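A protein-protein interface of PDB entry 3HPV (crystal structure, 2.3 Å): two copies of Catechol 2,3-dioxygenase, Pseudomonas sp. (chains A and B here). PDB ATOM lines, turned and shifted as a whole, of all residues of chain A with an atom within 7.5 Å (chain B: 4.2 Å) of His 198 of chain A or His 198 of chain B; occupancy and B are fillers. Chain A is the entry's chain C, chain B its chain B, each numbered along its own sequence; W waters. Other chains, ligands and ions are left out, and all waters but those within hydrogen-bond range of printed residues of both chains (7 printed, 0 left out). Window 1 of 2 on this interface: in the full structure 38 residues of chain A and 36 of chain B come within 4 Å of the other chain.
Hydrophobic or aromatic side chains of chain A within 4 Å of the printed part of chain B: Met 3, His 198, Tyr 276 and Pro 277.
Among the printed residues, 16 pairs touch across the chains.
Ser 195 of chain A touches none of the printed residues of chain B.
Printed residues of chain B within 4 Å of Ser 197 of chain A: Met 3 (3.8 Å) and His 198 (3.3 Å).
Of chain B, only Ser 197, His 198 and Lys 199 come within 4 Å of His 198 of chain A.
Pro 275 of chain A touches none of the printed residues of chain B.
Printed residues of chain B within 4 Å of Tyr 276 of chain A: Lys 199 (3.99 Å).
Of the printed residues of chain A, Met 3 of chain B touches Ala 2 (3.3 Å), Met 3 (3.4 Å), Ser 197 (3.8 Å) and Pro 277 (3.8 Å).
Of chain A, only Met 3 (3.95 Å), Ser 197 (3.3 Å), His 198 (3.1 Å) and Lys 199 (3.5 Å) come within 4 Å of His 198 of chain B.
The nearest residue of chain A that does not touch His 198 of chain B is Leu 7 of chain A (5.8 Å).
The nearest printed residue of chain B that does not touch Lys 199 of chain A is His 274 of chain B (6.6 Å).
Met 3 of chain A touches its own counterpart, Met 3 of chain B.
Met 3 of chain A touches Ser 197 of chain B, and with the chains exchanged Ser 197 of chain A touches Met 3 of chain B.
His 198 of chain B touches its own counterpart, His 198 of chain A.
His 198 of chain A touches Lys 199 of chain B, and with the chains exchanged Lys 199 of chain A touches His 198 of chain B.
8 positions are printed for both chains.
A ring nitrogen (NE2) of His 198 of chain B lies within hydrogen-bond range of a ring nitrogen (NE2) of His 198 of chain A (3.1 Å).
The side-chain sulfur of Met 3 of chain B lies close to the side-chain sulfur of Met 3 of chain A (3.4 Å).
N of Ser 197 of chain B is in hydrogen-bond range of OG of Ser 195 of chain B.
The backbone carbonyl oxygen (O) of Lys 199 of chain B lies within hydrogen-bond range of the side-chain hydroxyl (OG) of Ser 195 of chain B.
The side-chain hydroxyl of Tyr 176 of chain A sits at hydrogen-bond distance from the backbone carbonyl oxygen of Ser 197 of chain A (3.0 Å).
N of Ser 197 of chain A sits at hydrogen-bond distance from OG of Ser 195 of chain A (2.9 Å).
N of Lys 199 of chain A lies within hydrogen-bond range of OG of Ser 197 of chain A (3.2 Å).
The side-chain carboxylate (OD2) of Asp 202 of chain A sits at hydrogen-bond distance from the side-chain hydroxyl (OG) of Ser 197 of chain A, 2.8 Å away.
Among the printed residues, pairs that only touch across the chains: Ser 197 of chain A with His 198 of chain B (3.3 Å), His 198 of chain A with Ser 197 of chain B (3.3 Å), Ala 2 of chain A with Met 3 of chain B (3.3 Å), His 198 of chain A with Lys 199 of chain B (3.5 Å), Arg 8 of chain A with Tyr 276 of chain B (3.5 Å), Lys 199 of chain A with His 198 of chain B (3.5 Å), Met 3 of chain A with Ser 197 of chain B (3.7 Å), Pro 277 of chain A with Met 3 of chain B (3.8 Å), Lys 199 of chain A with Tyr 276 of chain B (3.8 Å), Leu 7 of chain A with Tyr 276 of chain B (3.8 Å), Ser 197 of chain A with Met 3 of chain B (3.8 Å), Gln 151 of chain A with His 274 of chain B (3.9 Å), Met 3 of chain A with His 198 of chain B (3.95 Å) and Tyr 276 of chain A with Lys 199 of chain B (3.99 Å).
Water W1 lies within hydrogen-bond range of O of Leu 7 of chain A (2.6 Å), OH of Tyr 276 of chain B (2.7 Å), OD1 of Asp 202 of chain A (3.0 Å) and OG of Ser 197 of chain A (3.4 Å).
Water W3 bridges the side-chain hydroxyl (OH) of Tyr 276 of chain A (2.8 Å) and the side-chain amino group (NZ) of Lys 199 of chain B (2.9 Å).
Water W5 lies within hydrogen-bond range of the backbone NH (N) of Met 3 of chain A (2.8 Å) and the backbone carbonyl oxygen (O) of Ser 197 of chain B (3.1 Å).
Water W2 lies within hydrogen-bond range of OH of Tyr 276 of chain B (2.8 Å), NZ of Lys 199 of chain A (2.9 Å) and OE1 of Gln 151 of chain A (3.1 Å).
Water W6 lies within hydrogen-bond range of the side-chain amide nitrogen (NE2) of Gln 151 of chain A and the side-chain hydroxyl (OH) of Tyr 276 of chain B.
Water W7 lies within hydrogen-bond range of NE2 of Gln 151 of chain A (3.3 Å) and ND1 of His 274 of chain B (3.5 Å).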
ATOM      1  N   ALA A   2     -25.545 -20.381 -38.573  1.00  0.00           N
ATOM      2  CA  ALA A   2     -25.156 -21.777 -38.892  1.00  0.00           C
ATOM      3  C   ALA A   2     -24.502 -22.468 -37.707  1.00  0.00           C
ATOM      4  O   ALA A   2     -23.935 -21.822 -36.816  1.00  0.00           O
ATOM      5  CB  ALA A   2     -24.213 -21.786 -40.066  1.00  0.00           C
ATOM      6  N   MET A   3     -24.598 -23.790 -37.702  1.00  0.00           N
ATOM      7  CA  MET A   3     -24.006 -24.612 -36.660  1.00  0.00           C
ATOM      8  C   MET A   3     -22.619 -25.051 -37.108  1.00  0.00           C
ATOM      9  O   MET A   3     -22.494 -25.924 -37.974  1.00  0.00           O
ATOM     10  CB  MET A   3     -24.867 -25.860 -36.394  1.00  0.00           C
ATOM     11  CG  MET A   3     -26.057 -25.627 -35.460  1.00  0.00           C
ATOM     12  SD  MET A   3     -25.540 -25.173 -33.793  1.00  0.00           S
ATOM     13  CE  MET A   3     -24.510 -26.625 -33.360  1.00  0.00           C
ATOM     14  N   LEU A   7     -20.928 -29.327 -32.764  1.00  0.00           N
ATOM     15  CA  LEU A   7     -22.346 -29.331 -33.027  1.00  0.00           C
ATOM     16  C   LEU A   7     -23.199 -29.765 -31.839  1.00  0.00           C
ATOM     17  O   LEU A   7     -23.953 -28.967 -31.300  1.00  0.00           O
ATOM     18  CB  LEU A   7     -22.654 -30.230 -34.225  1.00  0.00           C
ATOM     19  CG  LEU A   7     -21.917 -29.952 -35.538  1.00  0.00           C
ATOM     20  CD1 LEU A   7     -22.398 -30.956 -36.593  1.00  0.00           C
ATOM     21  CD2 LEU A   7     -22.163 -28.503 -35.989  1.00  0.00           C
ATOM     22  N   ARG A   8     -23.067 -31.016 -31.415  1.00  0.00           N
ATOM     23  CA  ARG A   8     -23.912 -31.538 -30.333  1.00  0.00           C
ATOM     24  C   ARG A   8     -23.284 -32.713 -29.601  1.00  0.00           C
ATOM     25  O   ARG A   8     -22.302 -33.298 -30.075  1.00  0.00           O
ATOM     26  CB  ARG A   8     -25.217 -32.056 -30.934  1.00  0.00           C
ATOM     27  CG  ARG A   8     -24.972 -33.286 -31.839  1.00  0.00           C
ATOM     28  CD  ARG A   8     -26.158 -33.571 -32.728  1.00  0.00           C
ATOM     29  NE  ARG A   8     -25.750 -33.756 -34.119  1.00  0.00           N
ATOM     30  CZ  ARG A   8     -25.285 -34.893 -34.600  1.00  0.00           C
ATOM     31  NH1 ARG A   8     -25.183 -35.928 -33.796  1.00  0.00           N
ATOM     32  NH2 ARG A   8     -24.919 -34.992 -35.864  1.00  0.00           N
ATOM     33  N   GLN A 151     -33.431 -37.847 -28.249  1.00  0.00           N
ATOM     34  CA  GLN A 151     -32.002 -37.616 -28.461  1.00  0.00           C
ATOM     35  C   GLN A 151     -31.213 -37.577 -27.148  1.00  0.00           C
ATOM     36  O   GLN A 151     -31.788 -37.472 -26.064  1.00  0.00           O
ATOM     37  CB  GLN A 151     -31.780 -36.293 -29.220  1.00  0.00           C
ATOM     38  CG  GLN A 151     -31.948 -34.998 -28.377  1.00  0.00           C
ATOM     39  CD  GLN A 151     -31.581 -33.699 -29.142  1.00  0.00           C
ATOM     40  OE1 GLN A 151     -31.111 -33.738 -30.278  1.00  0.00           O
ATOM     41  NE2 GLN A 151     -31.792 -32.550 -28.500  1.00  0.00           N
ATOM     42  N   TYR A 176     -20.817 -21.618 -24.586  1.00  0.00           N
ATOM     43  CA  TYR A 176     -21.077 -20.343 -23.926  1.00  0.00           C
ATOM     44  C   TYR A 176     -21.972 -20.589 -22.714  1.00  0.00           C
ATOM     45  O   TYR A 176     -22.664 -21.604 -22.656  1.00  0.00           O
ATOM     46  CB  TYR A 176     -21.696 -19.331 -24.902  1.00  0.00           C
ATOM     47  CG  TYR A 176     -23.112 -19.610 -25.363  1.00  0.00           C
ATOM     48  CD1 TYR A 176     -24.203 -18.918 -24.817  1.00  0.00           C
ATOM     49  CD2 TYR A 176     -23.365 -20.539 -26.367  1.00  0.00           C
ATOM     50  CE1 TYR A 176     -25.508 -19.154 -25.271  1.00  0.00           C
ATOM     51  CE2 TYR A 176     -24.653 -20.779 -26.820  1.00  0.00           C
ATOM     52  CZ  TYR A 176     -25.718 -20.088 -26.271  1.00  0.00           C
ATOM     53  OH  TYR A 176     -26.990 -20.353 -26.729  1.00  0.00           O
ATOM     54  N   VAL A 178     -25.035 -20.219 -20.288  1.00  0.00           N
ATOM     55  CA  VAL A 178     -26.446 -19.883 -20.370  1.00  0.00           C
ATOM     56  C   VAL A 178     -26.940 -19.615 -18.953  1.00  0.00           C
ATOM     57  O   VAL A 178     -27.667 -18.656 -18.704  1.00  0.00           O
ATOM     58  CB  VAL A 178     -27.276 -21.032 -20.994  1.00  0.00           C
ATOM     59  CG1 VAL A 178     -28.713 -20.589 -21.155  1.00  0.00           C
ATOM     60  CG2 VAL A 178     -26.681 -21.441 -22.356  1.00  0.00           C
ATOM     61  N   SER A 195     -23.728 -24.252 -23.371  1.00  0.00           N
ATOM     62  CA  SER A 195     -24.314 -24.574 -24.672  1.00  0.00           C
ATOM     63  C   SER A 195     -23.400 -24.268 -25.847  1.00  0.00           C
ATOM     64  O   SER A 195     -22.737 -23.237 -25.886  1.00  0.00           O
ATOM     65  CB  SER A 195     -25.599 -23.805 -24.910  1.00  0.00           C
ATOM     66  OG  SER A 195     -25.984 -23.975 -26.262  1.00  0.00           O
ATOM     67  N   CYS A 196     -23.384 -25.173 -26.812  1.00  0.00           N
ATOM     68  CA  CYS A 196     -22.593 -24.993 -28.013  1.00  0.00           C
ATOM     69  C   CYS A 196     -23.581 -24.926 -29.188  1.00  0.00           C
ATOM     70  O   CYS A 196     -23.241 -25.241 -30.326  1.00  0.00           O
ATOM     71  CB  CYS A 196     -21.634 -26.176 -28.192  1.00  0.00           C
ATOM     72  SG  CYS A 196     -22.446 -27.751 -28.547  1.00  0.00           S
ATOM     73  N   SER A 197     -24.804 -24.489 -28.908  1.00  0.00           N
ATOM     74  CA  SER A 197     -25.839 -24.422 -29.942  1.00  0.00           C
ATOM     75  C   SER A 197     -26.922 -23.447 -29.467  1.00  0.00           C
ATOM     76  O   SER A 197     -26.610 -22.452 -28.815  1.00  0.00           O
ATOM     77  CB  SER A 197     -26.425 -25.813 -30.090  1.00  0.00           C
ATOM     78  OG  SER A 197     -26.931 -26.218 -28.824  1.00  0.00           O
ATOM     79  N   HIS A 198     -28.186 -23.683 -29.816  1.00  0.00           N
ATOM     80  CA  HIS A 198     -29.191 -22.804 -29.245  1.00  0.00           C
ATOM     81  C   HIS A 198     -30.057 -23.560 -28.211  1.00  0.00           C
ATOM     82  O   HIS A 198     -31.198 -23.188 -27.915  1.00  0.00           O
ATOM     83  CB  HIS A 198     -30.034 -22.072 -30.308  1.00  0.00           C
ATOM     84  CG  HIS A 198     -30.823 -22.959 -31.210  1.00  0.00           C
ATOM     85  ND1 HIS A 198     -30.417 -23.264 -32.491  1.00  0.00           N
ATOM     86  CD2 HIS A 198     -32.010 -23.580 -31.036  1.00  0.00           C
ATOM     87  CE1 HIS A 198     -31.319 -24.036 -33.067  1.00  0.00           C
ATOM     88  NE2 HIS A 198     -32.297 -24.241 -32.205  1.00  0.00           N
ATOM     89  N   LYS A 199     -29.465 -24.616 -27.643  1.00  0.00           N
ATOM     90  CA  LYS A 199     -30.097 -25.420 -26.587  1.00  0.00           C
ATOM     91  C   LYS A 199     -29.720 -24.820 -25.227  1.00  0.00           C
ATOM     92  O   LYS A 199     -28.615 -24.263 -25.078  1.00  0.00           O
ATOM     93  CB  LYS A 199     -29.603 -26.860 -26.652  1.00  0.00           C
ATOM     94  CG  LYS A 199     -30.264 -27.706 -27.751  1.00  0.00           C
ATOM     95  CD  LYS A 199     -29.474 -28.995 -28.014  1.00  0.00           C
ATOM     96  CE  LYS A 199     -29.129 -29.695 -26.710  1.00  0.00           C
ATOM     97  NZ  LYS A 199     -28.267 -30.889 -26.923  1.00  0.00           N
ATOM     98  N   VAL A 200     -30.617 -24.899 -24.240  1.00  0.00           N
ATOM     99  CA  VAL A 200     -30.283 -24.352 -22.922  1.00  0.00           C
ATOM    100  C   VAL A 200     -28.881 -24.861 -22.577  1.00  0.00           C
ATOM    101  O   VAL A 200     -28.035 -24.088 -22.120  1.00  0.00           O
ATOM    102  CB  VAL A 200     -31.299 -24.759 -21.817  1.00  0.00           C
ATOM    103  CG1 VAL A 200     -30.906 -24.116 -20.498  1.00  0.00           C
ATOM    104  CG2 VAL A 200     -32.680 -24.278 -22.181  1.00  0.00           C
ATOM    105  N   HIS A 201     -28.628 -26.155 -22.789  1.00  0.00           N
ATOM    106  CA  HIS A 201     -27.284 -26.691 -22.570  1.00  0.00           C
ATOM    107  C   HIS A 201     -27.004 -28.052 -23.199  1.00  0.00           C
ATOM    108  O   HIS A 201     -27.887 -28.900 -23.305  1.00  0.00           O
ATOM    109  CB  HIS A 201     -26.910 -26.699 -21.073  1.00  0.00           C
ATOM    110  CG  HIS A 201     -27.580 -27.764 -20.259  1.00  0.00           C
ATOM    111  ND1 HIS A 201     -28.936 -28.002 -20.307  1.00  0.00           N
ATOM    112  CD2 HIS A 201     -27.086 -28.596 -19.308  1.00  0.00           C
ATOM    113  CE1 HIS A 201     -29.248 -28.931 -19.419  1.00  0.00           C
ATOM    114  NE2 HIS A 201     -28.143 -29.304 -18.798  1.00  0.00           N
ATOM    115  N   ASP A 202     -25.775 -28.230 -23.679  1.00  0.00           N
ATOM    116  CA  ASP A 202     -25.363 -29.510 -24.252  1.00  0.00           C
ATOM    117  C   ASP A 202     -24.502 -30.193 -23.169  1.00  0.00           C
ATOM    118  O   ASP A 202     -24.121 -31.367 -23.283  1.00  0.00           O
ATOM    119  CB  ASP A 202     -24.571 -29.289 -25.554  1.00  0.00           C
ATOM    120  CG  ASP A 202     -25.422 -28.630 -26.661  1.00  0.00           C
ATOM    121  OD1 ASP A 202     -26.346 -29.281 -27.175  1.00  0.00           O
ATOM    122  OD2 ASP A 202     -25.184 -27.463 -27.022  1.00  0.00           O
ATOM    123  N   TYR A 273     -36.106 -22.668 -22.688  1.00  0.00           N
ATOM    124  CA  TYR A 273     -36.146 -21.579 -23.651  1.00  0.00           C
ATOM    125  C   TYR A 273     -35.194 -21.825 -24.813  1.00  0.00           C
ATOM    126  O   TYR A 273     -34.717 -22.945 -25.013  1.00  0.00           O
ATOM    127  CB  TYR A 273     -35.837 -20.237 -22.970  1.00  0.00           C
ATOM    128  CG  TYR A 273     -34.636 -20.270 -22.050  1.00  0.00           C
ATOM    129  CD1 TYR A 273     -33.433 -19.659 -22.408  1.00  0.00           C
ATOM    130  CD2 TYR A 273     -34.704 -20.920 -20.813  1.00  0.00           C
ATOM    131  CE1 TYR A 273     -32.322 -19.696 -21.551  1.00  0.00           C
ATOM    132  CE2 TYR A 273     -33.611 -20.960 -19.957  1.00  0.00           C
ATOM    133  CZ  TYR A 273     -32.426 -20.345 -20.329  1.00  0.00           C
ATOM    134  OH  TYR A 273     -31.374 -20.353 -19.451  1.00  0.00           O
ATOM    135  N   HIS A 274     -34.921 -20.762 -25.569  1.00  0.00           N
ATOM    136  CA  HIS A 274     -34.087 -20.849 -26.753  1.00  0.00           C
ATOM    137  C   HIS A 274     -32.977 -19.802 -26.738  1.00  0.00           C
ATOM    138  O   HIS A 274     -33.075 -18.745 -27.364  1.00  0.00           O
ATOM    139  CB  HIS A 274     -34.984 -20.687 -27.977  1.00  0.00           C
ATOM    140  CG  HIS A 274     -36.186 -21.584 -27.953  1.00  0.00           C
ATOM    141  ND1 HIS A 274     -36.185 -22.851 -28.501  1.00  0.00           N
ATOM    142  CD2 HIS A 274     -37.404 -21.426 -27.379  1.00  0.00           C
ATOM    143  CE1 HIS A 274     -37.347 -23.434 -28.262  1.00  0.00           C
ATOM    144  NE2 HIS A 274     -38.104 -22.591 -27.582  1.00  0.00           N
ATOM    145  N   PRO A 275     -31.896 -20.091 -26.021  1.00  0.00           N
ATOM    146  CA  PRO A 275     -30.782 -19.147 -25.944  1.00  0.00           C
ATOM    147  C   PRO A 275     -29.861 -19.174 -27.154  1.00  0.00           C
ATOM    148  O   PRO A 275     -29.782 -20.176 -27.882  1.00  0.00           O
ATOM    149  CB  PRO A 275     -30.067 -19.581 -24.676  1.00  0.00           C
ATOM    150  CG  PRO A 275     -30.201 -21.079 -24.749  1.00  0.00           C
ATOM    151  CD  PRO A 275     -31.656 -21.262 -25.161  1.00  0.00           C
ATOM    152  N   TYR A 276     -29.172 -18.057 -27.365  1.00  0.00           N
ATOM    153  CA  TYR A 276     -28.227 -17.929 -28.461  1.00  0.00           C
ATOM    154  C   TYR A 276     -26.939 -17.291 -27.915  1.00  0.00           C
ATOM    155  O   TYR A 276     -26.952 -16.647 -26.854  1.00  0.00           O
ATOM    156  CB  TYR A 276     -28.845 -17.104 -29.589  1.00  0.00           C
ATOM    157  CG  TYR A 276     -29.892 -17.843 -30.391  1.00  0.00           C
ATOM    158  CD1 TYR A 276     -29.567 -18.428 -31.601  1.00  0.00           C
ATOM    159  CD2 TYR A 276     -31.218 -17.921 -29.956  1.00  0.00           C
ATOM    160  CE1 TYR A 276     -30.524 -19.066 -32.384  1.00  0.00           C
ATOM    161  CE2 TYR A 276     -32.202 -18.558 -30.727  1.00  0.00           C
ATOM    162  CZ  TYR A 276     -31.846 -19.124 -31.949  1.00  0.00           C
ATOM    163  OH  TYR A 276     -32.790 -19.691 -32.771  1.00  0.00           O
ATOM    164  N   PRO A 277     -25.808 -17.468 -28.625  1.00  0.00           N
ATOM    165  CA  PRO A 277     -24.539 -16.903 -28.161  1.00  0.00           C
ATOM    166  C   PRO A 277     -24.529 -15.395 -27.853  1.00  0.00           C
ATOM    167  O   PRO A 277     -23.635 -14.916 -27.139  1.00  0.00           O
ATOM    168  CB  PRO A 277     -23.560 -17.289 -29.272  1.00  0.00           C
ATOM    169  CG  PRO A 277     -24.175 -18.529 -29.874  1.00  0.00           C
ATOM    170  CD  PRO A 277     -25.635 -18.160 -29.913  1.00  0.00           C
ATOM    171  N   MET B   3     -23.159 -21.680 -32.647  1.00  0.00           N
ATOM    172  CA  MET B   3     -24.039 -21.041 -33.619  1.00  0.00           C
ATOM    173  C   MET B   3     -23.239 -19.852 -34.154  1.00  0.00           C
ATOM    174  O   MET B   3     -22.890 -18.941 -33.417  1.00  0.00           O
ATOM    175  CB  MET B   3     -25.340 -20.578 -32.963  1.00  0.00           C
ATOM    176  CG  MET B   3     -26.399 -21.677 -32.838  1.00  0.00           C
ATOM    177  SD  MET B   3     -27.010 -22.217 -34.447  1.00  0.00           S
ATOM    178  CE  MET B   3     -27.768 -20.685 -35.045  1.00  0.00           C
ATOM    179  N   SER B 195     -32.387 -24.403 -43.021  1.00  0.00           N
ATOM    180  CA  SER B 195     -32.002 -24.096 -41.640  1.00  0.00           C
ATOM    181  C   SER B 195     -30.598 -23.489 -41.553  1.00  0.00           C
ATOM    182  O   SER B 195     -29.733 -23.772 -42.373  1.00  0.00           O
ATOM    183  CB  SER B 195     -32.042 -25.340 -40.741  1.00  0.00           C
ATOM    184  OG  SER B 195     -31.471 -25.057 -39.456  1.00  0.00           O
ATOM    185  N   SER B 197     -29.466 -23.309 -38.264  1.00  0.00           N
ATOM    186  CA  SER B 197     -29.330 -23.722 -36.856  1.00  0.00           C
ATOM    187  C   SER B 197     -29.578 -25.238 -36.761  1.00  0.00           C
ATOM    188  O   SER B 197     -29.094 -26.002 -37.600  1.00  0.00           O
ATOM    189  CB  SER B 197     -30.386 -22.996 -36.043  1.00  0.00           C
ATOM    190  OG  SER B 197     -31.643 -23.220 -36.658  1.00  0.00           O
ATOM    191  N   HIS B 198     -30.299 -25.670 -35.725  1.00  0.00           N
ATOM    192  CA  HIS B 198     -30.652 -27.077 -35.615  1.00  0.00           C
ATOM    193  C   HIS B 198     -32.175 -27.197 -35.463  1.00  0.00           C
ATOM    194  O   HIS B 198     -32.688 -28.101 -34.813  1.00  0.00           O
ATOM    195  CB  HIS B 198     -29.892 -27.829 -34.490  1.00  0.00           C
ATOM    196  CG  HIS B 198     -30.035 -27.241 -33.118  1.00  0.00           C
ATOM    197  ND1 HIS B 198     -29.065 -26.451 -32.540  1.00  0.00           N
ATOM    198  CD2 HIS B 198     -31.022 -27.349 -32.200  1.00  0.00           C
ATOM    199  CE1 HIS B 198     -29.448 -26.094 -31.328  1.00  0.00           C
ATOM    200  NE2 HIS B 198     -30.632 -26.627 -31.097  1.00  0.00           N
ATOM    201  N   LYS B 199     -32.872 -26.238 -36.071  1.00  0.00           N
ATOM    202  CA  LYS B 199     -34.325 -26.194 -36.115  1.00  0.00           C
ATOM    203  C   LYS B 199     -34.664 -26.760 -37.495  1.00  0.00           C
ATOM    204  O   LYS B 199     -33.841 -26.696 -38.415  1.00  0.00           O
ATOM    205  CB  LYS B 199     -34.838 -24.746 -36.051  1.00  0.00           C
ATOM    206  CG  LYS B 199     -34.686 -24.022 -34.696  1.00  0.00           C
ATOM    207  CD  LYS B 199     -34.674 -22.488 -34.898  1.00  0.00           C
ATOM    208  CE  LYS B 199     -35.946 -21.980 -35.588  1.00  0.00           C
ATOM    209  NZ  LYS B 199     -35.817 -20.569 -36.071  1.00  0.00           N
ATOM    210  N   HIS B 274     -34.990 -32.402 -34.495  1.00  0.00           N
ATOM    211  CA  HIS B 274     -33.786 -31.604 -34.262  1.00  0.00           C
ATOM    212  C   HIS B 274     -32.625 -31.889 -35.217  1.00  0.00           C
ATOM    213  O   HIS B 274     -31.630 -32.513 -34.835  1.00  0.00           O
ATOM    214  CB  HIS B 274     -33.358 -31.815 -32.817  1.00  0.00           C
ATOM    215  CG  HIS B 274     -34.512 -31.827 -31.871  1.00  0.00           C
ATOM    216  ND1 HIS B 274     -35.019 -30.678 -31.298  1.00  0.00           N
ATOM    217  CD2 HIS B 274     -35.325 -32.837 -31.474  1.00  0.00           C
ATOM    218  CE1 HIS B 274     -36.094 -30.978 -30.594  1.00  0.00           C
ATOM    219  NE2 HIS B 274     -36.302 -32.281 -30.684  1.00  0.00           N
ATOM    220  N   PRO B 275     -32.737 -31.420 -36.471  1.00  0.00           N
ATOM    221  CA  PRO B 275     -31.718 -31.610 -37.506  1.00  0.00           C
ATOM    222  C   PRO B 275     -30.451 -30.781 -37.316  1.00  0.00           C
ATOM    223  O   PRO B 275     -30.464 -29.731 -36.654  1.00  0.00           O
ATOM    224  CB  PRO B 275     -32.464 -31.228 -38.787  1.00  0.00           C
ATOM    225  CG  PRO B 275     -33.338 -30.097 -38.308  1.00  0.00           C
ATOM    226  CD  PRO B 275     -33.884 -30.657 -37.004  1.00  0.00           C
ATOM    227  N   TYR B 276     -29.357 -31.263 -37.909  1.00  0.00           N
ATOM    228  CA  TYR B 276     -28.063 -30.566 -37.852  1.00  0.00           C
ATOM    229  C   TYR B 276     -27.432 -30.538 -39.233  1.00  0.00           C
ATOM    230  O   TYR B 276     -27.807 -31.333 -40.090  1.00  0.00           O
ATOM    231  CB  TYR B 276     -27.125 -31.267 -36.886  1.00  0.00           C
ATOM    232  CG  TYR B 276     -27.475 -31.046 -35.445  1.00  0.00           C
ATOM    233  CD1 TYR B 276     -26.746 -30.137 -34.669  1.00  0.00           C
ATOM    234  CD2 TYR B 276     -28.544 -31.737 -34.844  1.00  0.00           C
ATOM    235  CE1 TYR B 276     -27.056 -29.915 -33.332  1.00  0.00           C
ATOM    236  CE2 TYR B 276     -28.873 -31.524 -33.491  1.00  0.00           C
ATOM    237  CZ  TYR B 276     -28.124 -30.609 -32.740  1.00  0.00           C
ATOM    238  OH  TYR B 276     -28.434 -30.367 -31.411  1.00  0.00           O
HETATM  239  O   HOH W   1     -26.282 -29.289 -30.148  1.00  0.00           O
HETATM  240  O   HOH W   2     -28.414 -32.372 -29.417  1.00  0.00           O
HETATM  241  O   HOH W   3     -35.200 -18.852 -33.821  1.00  0.00           O
HETATM  242  O   HOH W   4     -32.190 -20.256 -35.380  1.00  0.00           O
HETATM  243  O   HOH W   5     -26.634 -25.013 -39.119  1.00  0.00           O
HETATM  244  O   HOH W   6     -31.200 -30.653 -30.549  1.00  0.00           O
HETATM  245  O   HOH W   7     -32.902 -29.478 -28.833  1.00  0.00           O
